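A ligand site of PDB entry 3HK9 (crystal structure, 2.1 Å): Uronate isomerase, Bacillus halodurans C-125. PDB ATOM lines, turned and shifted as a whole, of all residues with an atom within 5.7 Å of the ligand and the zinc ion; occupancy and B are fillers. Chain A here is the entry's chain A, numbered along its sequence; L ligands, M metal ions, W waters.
The side-chain hydroxyl (OH) of Tyr 50 is in hydrogen-bond range of an oxygen (O7) of the ligand, at 2.6 Å. O6 of the ligand is in hydrogen-bond range of NE of Arg 357, at 2.6 Å. The guanidinium group (NH2) of Arg 170 lies within salt-bridge range of an oxygen (O1) of the ligand (2.7 Å). The indole nitrogen (NE1) of Trp 325 sits close to an oxygen (O3) of the ligand, 2.8 Å away. A ring nitrogen (NE2) of His 49 lies within hydrogen-bond range of an oxygen (O5) of the ligand, at 2.9 Å.
A ring nitrogen (ND1) of His 26 sits close to the side-chain hydroxyl (OG1) of Thr 143, 3.4 Å away. OD2 of Asp 355 sits close to NE1 of Trp 325. A ring nitrogen (NE2) of His 353 lies within hydrogen-bond range of the side-chain carboxylate (OD2) of Asp 355 (3.4 Å). The side-chain hydroxyl (OG) of Ser 223 sits close to the guanidinium group (NH2) of Arg 170 (3.3 Å). The guanidinium group (NE) of Arg 170 is in salt-bridge range of the side-chain carboxylate (OD1) of Asp 172 (2.6 Å). ND1 of His 49 sits at hydrogen-bond distance from O of Asp 271 (3.3 Å). The side-chain carboxylate (OD2) of Asp 172 sits at hydrogen-bond distance from the side-chain hydroxyl (OG) of Ser 223 (2.7 Å).
Residues that only touch the ligand: Ser 223, Met 258 and Trp 326.
Three residues have an atom within 4 Å of the zinc ion: His 26, His 28 and Asp 355. The nearest printed residue that does not touch the zinc ion is Trp 325 (4.05 Å).
The zinc ion is bound by O3 of the ligand (2.0 Å), NE2 of His 28 (2.2 Å), NE2 of His 26 (2.2 Å), OD1 of Asp 355 (2.2 Å) and O2 of the ligand (2.3 Å). The zinc ion has five donor atoms within binding distance.
Water W2 lies within hydrogen-bond range of the side-chain carboxylate (OD2) of Asp 274 (2.6 Å), the backbone carbonyl oxygen (O) of Asp 271 (2.8 Å) and an oxygen (O5) of the ligand (2.8 Å). Water W1 lies within hydrogen-bond range of an oxygen (O1) of the ligand, the side-chain amino group of Lys 263 and the side-chain hydroxyl of Ser 223.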
ATOM      1  N   HIS A  26      27.024 -31.615  21.832  1.00  0.00           N
ATOM      2  CA  HIS A  26      26.479 -30.410  22.455  1.00  0.00           C
ATOM      3  C   HIS A  26      27.386 -29.209  22.206  1.00  0.00           C
ATOM      4  O   HIS A  26      28.511 -29.153  22.693  1.00  0.00           O
ATOM      5  CB  HIS A  26      26.250 -30.526  23.970  1.00  0.00           C
ATOM      6  CG  HIS A  26      25.747 -29.253  24.595  1.00  0.00           C
ATOM      7  ND1 HIS A  26      24.621 -28.596  24.140  1.00  0.00           N
ATOM      8  CD2 HIS A  26      26.248 -28.473  25.590  1.00  0.00           C
ATOM      9  CE1 HIS A  26      24.449 -27.479  24.828  1.00  0.00           C
ATOM     10  NE2 HIS A  26      25.424 -27.382  25.715  1.00  0.00           N
ATOM     11  N   THR A  27      26.860 -28.262  21.437  1.00  0.00           N
ATOM     12  CA  THR A  27      27.587 -27.042  21.089  1.00  0.00           C
ATOM     13  C   THR A  27      26.574 -25.915  20.944  1.00  0.00           C
ATOM     14  O   THR A  27      25.364 -26.144  20.948  1.00  0.00           O
ATOM     15  CB  THR A  27      28.294 -27.172  19.731  1.00  0.00           C
ATOM     16  OG1 THR A  27      27.328 -27.067  18.679  1.00  0.00           O
ATOM     17  CG2 THR A  27      29.009 -28.513  19.612  1.00  0.00           C
ATOM     18  N   HIS A  28      27.088 -24.694  20.790  1.00  0.00           N
ATOM     19  CA  HIS A  28      26.239 -23.530  20.587  1.00  0.00           C
ATOM     20  C   HIS A  28      26.620 -22.957  19.230  1.00  0.00           C
ATOM     21  O   HIS A  28      26.645 -21.734  19.032  1.00  0.00           O
ATOM     22  CB  HIS A  28      26.460 -22.521  21.703  1.00  0.00           C
ATOM     23  CG  HIS A  28      25.955 -22.991  23.030  1.00  0.00           C
ATOM     24  ND1 HIS A  28      24.629 -22.972  23.368  1.00  0.00           N
ATOM     25  CD2 HIS A  28      26.602 -23.587  24.070  1.00  0.00           C
ATOM     26  CE1 HIS A  28      24.467 -23.528  24.554  1.00  0.00           C
ATOM     27  NE2 HIS A  28      25.651 -23.906  24.999  1.00  0.00           N
ATOM     28  N   TYR A  48      34.619 -14.524  24.333  1.00  0.00           N
ATOM     29  CA  TYR A  48      33.887 -15.690  24.833  1.00  0.00           C
ATOM     30  C   TYR A  48      33.572 -15.263  26.272  1.00  0.00           C
ATOM     31  O   TYR A  48      34.414 -14.647  26.928  1.00  0.00           O
ATOM     32  CB  TYR A  48      34.822 -16.897  24.788  1.00  0.00           C
ATOM     33  CG  TYR A  48      34.310 -18.215  25.307  1.00  0.00           C
ATOM     34  CD1 TYR A  48      33.021 -18.660  25.029  1.00  0.00           C
ATOM     35  CD2 TYR A  48      35.162 -19.076  25.995  1.00  0.00           C
ATOM     36  CE1 TYR A  48      32.605 -19.962  25.407  1.00  0.00           C
ATOM     37  CE2 TYR A  48      34.764 -20.361  26.377  1.00  0.00           C
ATOM     38  CZ  TYR A  48      33.491 -20.795  26.078  1.00  0.00           C
ATOM     39  OH  TYR A  48      33.133 -22.083  26.402  1.00  0.00           O
ATOM     40  N   HIS A  49      32.388 -15.586  26.788  1.00  0.00           N
ATOM     41  CA  HIS A  49      32.060 -15.129  28.136  1.00  0.00           C
ATOM     42  C   HIS A  49      32.981 -15.629  29.244  1.00  0.00           C
ATOM     43  O   HIS A  49      33.076 -14.994  30.306  1.00  0.00           O
ATOM     44  CB  HIS A  49      30.569 -15.357  28.458  1.00  0.00           C
ATOM     45  CG  HIS A  49      30.178 -16.773  28.736  1.00  0.00           C
ATOM     46  ND1 HIS A  49      30.380 -17.381  29.951  1.00  0.00           N
ATOM     47  CD2 HIS A  49      29.481 -17.669  27.994  1.00  0.00           C
ATOM     48  CE1 HIS A  49      29.823 -18.584  29.955  1.00  0.00           C
ATOM     49  NE2 HIS A  49      29.267 -18.774  28.778  1.00  0.00           N
ATOM     50  N   TYR A  50      33.689 -16.734  29.003  1.00  0.00           N
ATOM     51  CA  TYR A  50      34.621 -17.255  30.001  1.00  0.00           C
ATOM     52  C   TYR A  50      35.698 -16.203  30.238  1.00  0.00           C
ATOM     53  O   TYR A  50      36.137 -15.986  31.370  1.00  0.00           O
ATOM     54  CB  TYR A  50      35.314 -18.543  29.495  1.00  0.00           C
ATOM     55  CG  TYR A  50      34.501 -19.816  29.575  1.00  0.00           C
ATOM     56  CD1 TYR A  50      33.118 -19.823  29.333  1.00  0.00           C
ATOM     57  CD2 TYR A  50      35.124 -21.042  29.843  1.00  0.00           C
ATOM     58  CE1 TYR A  50      32.390 -21.028  29.340  1.00  0.00           C
ATOM     59  CE2 TYR A  50      34.401 -22.242  29.856  1.00  0.00           C
ATOM     60  CZ  TYR A  50      33.043 -22.227  29.607  1.00  0.00           C
ATOM     61  OH  TYR A  50      32.330 -23.415  29.634  1.00  0.00           O
ATOM     62  N   THR A 143      22.253 -26.254  19.653  1.00  0.00           N
ATOM     63  CA  THR A 143      21.291 -26.038  20.715  1.00  0.00           C
ATOM     64  C   THR A 143      20.293 -25.114  20.046  1.00  0.00           C
ATOM     65  O   THR A 143      20.571 -23.919  19.843  1.00  0.00           O
ATOM     66  CB  THR A 143      21.907 -25.323  21.938  1.00  0.00           C
ATOM     67  OG1 THR A 143      22.879 -26.163  22.554  1.00  0.00           O
ATOM     68  CG2 THR A 143      20.814 -24.994  22.951  1.00  0.00           C
ATOM     69  N   ARG A 170      15.995 -27.374  22.490  1.00  0.00           N
ATOM     70  CA  ARG A 170      16.213 -26.807  23.823  1.00  0.00           C
ATOM     71  C   ARG A 170      14.884 -26.251  24.359  1.00  0.00           C
ATOM     72  O   ARG A 170      14.211 -25.464  23.682  1.00  0.00           O
ATOM     73  CB  ARG A 170      17.285 -25.725  23.723  1.00  0.00           C
ATOM     74  CG  ARG A 170      17.840 -25.262  25.056  1.00  0.00           C
ATOM     75  CD  ARG A 170      18.361 -26.425  25.908  1.00  0.00           C
ATOM     76  NE  ARG A 170      18.846 -25.903  27.180  1.00  0.00           N
ATOM     77  CZ  ARG A 170      20.106 -25.514  27.406  1.00  0.00           C
ATOM     78  NH1 ARG A 170      21.026 -25.612  26.453  1.00  0.00           N
ATOM     79  NH2 ARG A 170      20.420 -24.967  28.569  1.00  0.00           N
ATOM     80  N   ASP A 172      14.308 -24.842  27.876  1.00  0.00           N
ATOM     81  CA  ASP A 172      14.380 -24.128  29.156  1.00  0.00           C
ATOM     82  C   ASP A 172      13.180 -23.217  29.477  1.00  0.00           C
ATOM     83  O   ASP A 172      12.638 -23.263  30.586  1.00  0.00           O
ATOM     84  CB  ASP A 172      15.686 -23.320  29.245  1.00  0.00           C
ATOM     85  CG  ASP A 172      16.927 -24.213  29.284  1.00  0.00           C
ATOM     86  OD1 ASP A 172      16.838 -25.368  28.811  1.00  0.00           O
ATOM     87  OD2 ASP A 172      18.001 -23.767  29.756  1.00  0.00           O
ATOM     88  N   SER A 223      18.399 -27.140  30.795  1.00  0.00           N
ATOM     89  CA  SER A 223      19.418 -26.973  31.831  1.00  0.00           C
ATOM     90  C   SER A 223      18.569 -26.761  33.084  1.00  0.00           C
ATOM     91  O   SER A 223      17.532 -26.101  33.028  1.00  0.00           O
ATOM     92  CB  SER A 223      20.332 -25.766  31.571  1.00  0.00           C
ATOM     93  OG  SER A 223      19.652 -24.533  31.727  1.00  0.00           O
ATOM     94  N   MET A 258      20.907 -31.099  31.803  1.00  0.00           N
ATOM     95  CA  MET A 258      22.193 -30.563  32.214  1.00  0.00           C
ATOM     96  C   MET A 258      21.894 -29.893  33.554  1.00  0.00           C
ATOM     97  O   MET A 258      21.338 -28.788  33.612  1.00  0.00           O
ATOM     98  CB  MET A 258      22.680 -29.577  31.160  1.00  0.00           C
ATOM     99  CG  MET A 258      22.459 -30.102  29.750  1.00  0.00           C
ATOM    100  SD  MET A 258      23.705 -29.578  28.586  1.00  0.00           S
ATOM    101  CE  MET A 258      23.107 -27.985  28.166  1.00  0.00           C
ATOM    102  N   LYS A 263      21.303 -19.867  37.545  1.00  0.00           N
ATOM    103  CA  LYS A 263      21.210 -18.735  36.626  1.00  0.00           C
ATOM    104  C   LYS A 263      21.341 -17.340  37.222  1.00  0.00           C
ATOM    105  O   LYS A 263      20.839 -17.050  38.299  1.00  0.00           O
ATOM    106  CB  LYS A 263      19.897 -18.820  35.834  1.00  0.00           C
ATOM    107  CG  LYS A 263      19.714 -20.096  35.039  1.00  0.00           C
ATOM    108  CD  LYS A 263      20.816 -20.302  34.004  1.00  0.00           C
ATOM    109  CE  LYS A 263      20.790 -19.248  32.911  1.00  0.00           C
ATOM    110  NZ  LYS A 263      21.851 -19.501  31.886  1.00  0.00           N
ATOM    111  N   ASP A 271      25.922 -13.488  30.123  1.00  0.00           N
ATOM    112  CA  ASP A 271      26.188 -14.920  29.996  1.00  0.00           C
ATOM    113  C   ASP A 271      27.289 -15.413  30.926  1.00  0.00           C
ATOM    114  O   ASP A 271      27.435 -16.605  31.156  1.00  0.00           O
ATOM    115  CB  ASP A 271      26.557 -15.260  28.548  1.00  0.00           C
ATOM    116  CG  ASP A 271      25.356 -15.283  27.623  1.00  0.00           C
ATOM    117  OD1 ASP A 271      24.224 -15.423  28.123  1.00  0.00           O
ATOM    118  OD2 ASP A 271      25.558 -15.179  26.391  1.00  0.00           O
ATOM    119  N   ASP A 274      26.516 -16.868  35.481  1.00  0.00           N
ATOM    120  CA  ASP A 274      25.873 -18.061  36.015  1.00  0.00           C
ATOM    121  C   ASP A 274      26.779 -18.781  37.023  1.00  0.00           C
ATOM    122  O   ASP A 274      28.004 -18.836  36.848  1.00  0.00           O
ATOM    123  CB  ASP A 274      25.484 -19.036  34.884  1.00  0.00           C
ATOM    124  CG  ASP A 274      24.421 -18.443  33.931  1.00  0.00           C
ATOM    125  OD1 ASP A 274      23.615 -17.598  34.374  1.00  0.00           O
ATOM    126  OD2 ASP A 274      24.391 -18.842  32.755  1.00  0.00           O
ATOM    127  N   TRP A 325      31.126 -30.681  31.582  1.00  0.00           N
ATOM    128  CA  TRP A 325      30.449 -29.425  31.327  1.00  0.00           C
ATOM    129  C   TRP A 325      30.866 -28.154  32.066  1.00  0.00           C
ATOM    130  O   TRP A 325      30.959 -28.129  33.293  1.00  0.00           O
ATOM    131  CB  TRP A 325      28.956 -29.663  31.555  1.00  0.00           C
ATOM    132  CG  TRP A 325      28.050 -28.508  31.235  1.00  0.00           C
ATOM    133  CD1 TRP A 325      28.125 -27.668  30.164  1.00  0.00           C
ATOM    134  CD2 TRP A 325      26.838 -28.154  31.937  1.00  0.00           C
ATOM    135  NE1 TRP A 325      27.046 -26.815  30.150  1.00  0.00           N
ATOM    136  CE2 TRP A 325      26.243 -27.094  31.224  1.00  0.00           C
ATOM    137  CE3 TRP A 325      26.217 -28.628  33.095  1.00  0.00           C
ATOM    138  CZ2 TRP A 325      25.038 -26.494  31.636  1.00  0.00           C
ATOM    139  CZ3 TRP A 325      25.007 -28.035  33.500  1.00  0.00           C
ATOM    140  CH2 TRP A 325      24.447 -26.984  32.771  1.00  0.00           C
ATOM    141  N   TRP A 326      31.133 -27.109  31.281  1.00  0.00           N
ATOM    142  CA  TRP A 326      31.397 -25.778  31.808  1.00  0.00           C
ATOM    143  C   TRP A 326      32.550 -25.656  32.816  1.00  0.00           C
ATOM    144  O   TRP A 326      33.721 -25.651  32.449  1.00  0.00           O
ATOM    145  CB  TRP A 326      30.099 -25.309  32.457  1.00  0.00           C
ATOM    146  CG  TRP A 326      29.795 -23.861  32.447  1.00  0.00           C
ATOM    147  CD1 TRP A 326      30.687 -22.827  32.425  1.00  0.00           C
ATOM    148  CD2 TRP A 326      28.501 -23.275  32.560  1.00  0.00           C
ATOM    149  NE1 TRP A 326      30.017 -21.624  32.526  1.00  0.00           N
ATOM    150  CE2 TRP A 326      28.671 -21.876  32.616  1.00  0.00           C
ATOM    151  CE3 TRP A 326      27.207 -23.806  32.629  1.00  0.00           C
ATOM    152  CZ2 TRP A 326      27.592 -20.999  32.731  1.00  0.00           C
ATOM    153  CZ3 TRP A 326      26.137 -22.939  32.746  1.00  0.00           C
ATOM    154  CH2 TRP A 326      26.338 -21.541  32.796  1.00  0.00           C
ATOM    155  N   HIS A 353      32.227 -33.138  25.215  1.00  0.00           N
ATOM    156  CA  HIS A 353      31.528 -32.330  24.210  1.00  0.00           C
ATOM    157  C   HIS A 353      32.256 -30.988  24.295  1.00  0.00           C
ATOM    158  O   HIS A 353      32.876 -30.700  25.313  1.00  0.00           O
ATOM    159  CB  HIS A 353      30.024 -32.184  24.489  1.00  0.00           C
ATOM    160  CG  HIS A 353      29.682 -31.364  25.702  1.00  0.00           C
ATOM    161  ND1 HIS A 353      29.566 -31.913  26.956  1.00  0.00           N
ATOM    162  CD2 HIS A 353      29.395 -30.051  25.825  1.00  0.00           C
ATOM    163  CE1 HIS A 353      29.227 -30.961  27.814  1.00  0.00           C
ATOM    164  NE2 HIS A 353      29.113 -29.819  27.156  1.00  0.00           N
ATOM    165  N   ASP A 355      30.853 -27.719  23.621  1.00  0.00           N
ATOM    166  CA  ASP A 355      30.014 -26.647  24.132  1.00  0.00           C
ATOM    167  C   ASP A 355      30.477 -25.373  23.416  1.00  0.00           C
ATOM    168  O   ASP A 355      30.338 -24.266  23.941  1.00  0.00           O
ATOM    169  CB  ASP A 355      30.224 -26.475  25.644  1.00  0.00           C
ATOM    170  CG  ASP A 355      28.950 -26.076  26.381  1.00  0.00           C
ATOM    171  OD1 ASP A 355      28.082 -25.420  25.775  1.00  0.00           O
ATOM    172  OD2 ASP A 355      28.833 -26.423  27.567  1.00  0.00           O
ATOM    173  N   ARG A 357      30.884 -22.046  21.490  1.00  0.00           N
ATOM    174  CA  ARG A 357      30.021 -20.892  21.261  1.00  0.00           C
ATOM    175  C   ARG A 357      30.627 -20.141  20.085  1.00  0.00           C
ATOM    176  O   ARG A 357      29.950 -19.389  19.396  1.00  0.00           O
ATOM    177  CB  ARG A 357      29.987 -19.992  22.500  1.00  0.00           C
ATOM    178  CG  ARG A 357      28.993 -20.415  23.564  1.00  0.00           C
ATOM    179  CD  ARG A 357      28.997 -19.471  24.740  1.00  0.00           C
ATOM    180  NE  ARG A 357      27.868 -19.679  25.641  1.00  0.00           N
ATOM    181  CZ  ARG A 357      26.609 -19.338  25.370  1.00  0.00           C
ATOM    182  NH1 ARG A 357      26.313 -18.757  24.215  1.00  0.00           N
ATOM    183  NH2 ARG A 357      25.646 -19.570  26.249  1.00  0.00           N
HETATM  184  O1  LIG L   1      22.991 -24.479  29.264  1.00  0.00           O
HETATM  185  C1  LIG L   1      23.948 -24.586  28.441  1.00  0.00           C
HETATM  186  O2  LIG L   1      23.875 -25.122  27.324  1.00  0.00           O
HETATM  187  C2  LIG L   1      25.290 -24.017  28.904  1.00  0.00           C
HETATM  188  O3  LIG L   1      26.332 -24.828  28.340  1.00  0.00           O
HETATM  189  C3  LIG L   1      25.517 -22.540  28.465  1.00  0.00           C
HETATM  190  O4  LIG L   1      24.467 -21.765  29.080  1.00  0.00           O
HETATM  191  C4  LIG L   1      26.889 -21.933  28.874  1.00  0.00           C
HETATM  192  O5  LIG L   1      26.913 -20.504  28.679  1.00  0.00           O
HETATM  193  C5  LIG L   1      28.046 -22.599  28.089  1.00  0.00           C
HETATM  194  O6  LIG L   1      28.519 -21.763  27.040  1.00  0.00           O
HETATM  195  C6  LIG L   1      29.195 -22.966  29.027  1.00  0.00           C
HETATM  196  O7  LIG L   1      29.934 -23.933  28.796  1.00  0.00           O
HETATM  197 ZN    ZN M   1      25.995 -25.406  26.504  1.00  0.00          ZN
HETATM  198  O   HOH W   1      22.388 -22.442  31.306  1.00  0.00           O
HETATM  199  O   HOH W   2      25.686 -18.737  30.542  1.00  0.00           O
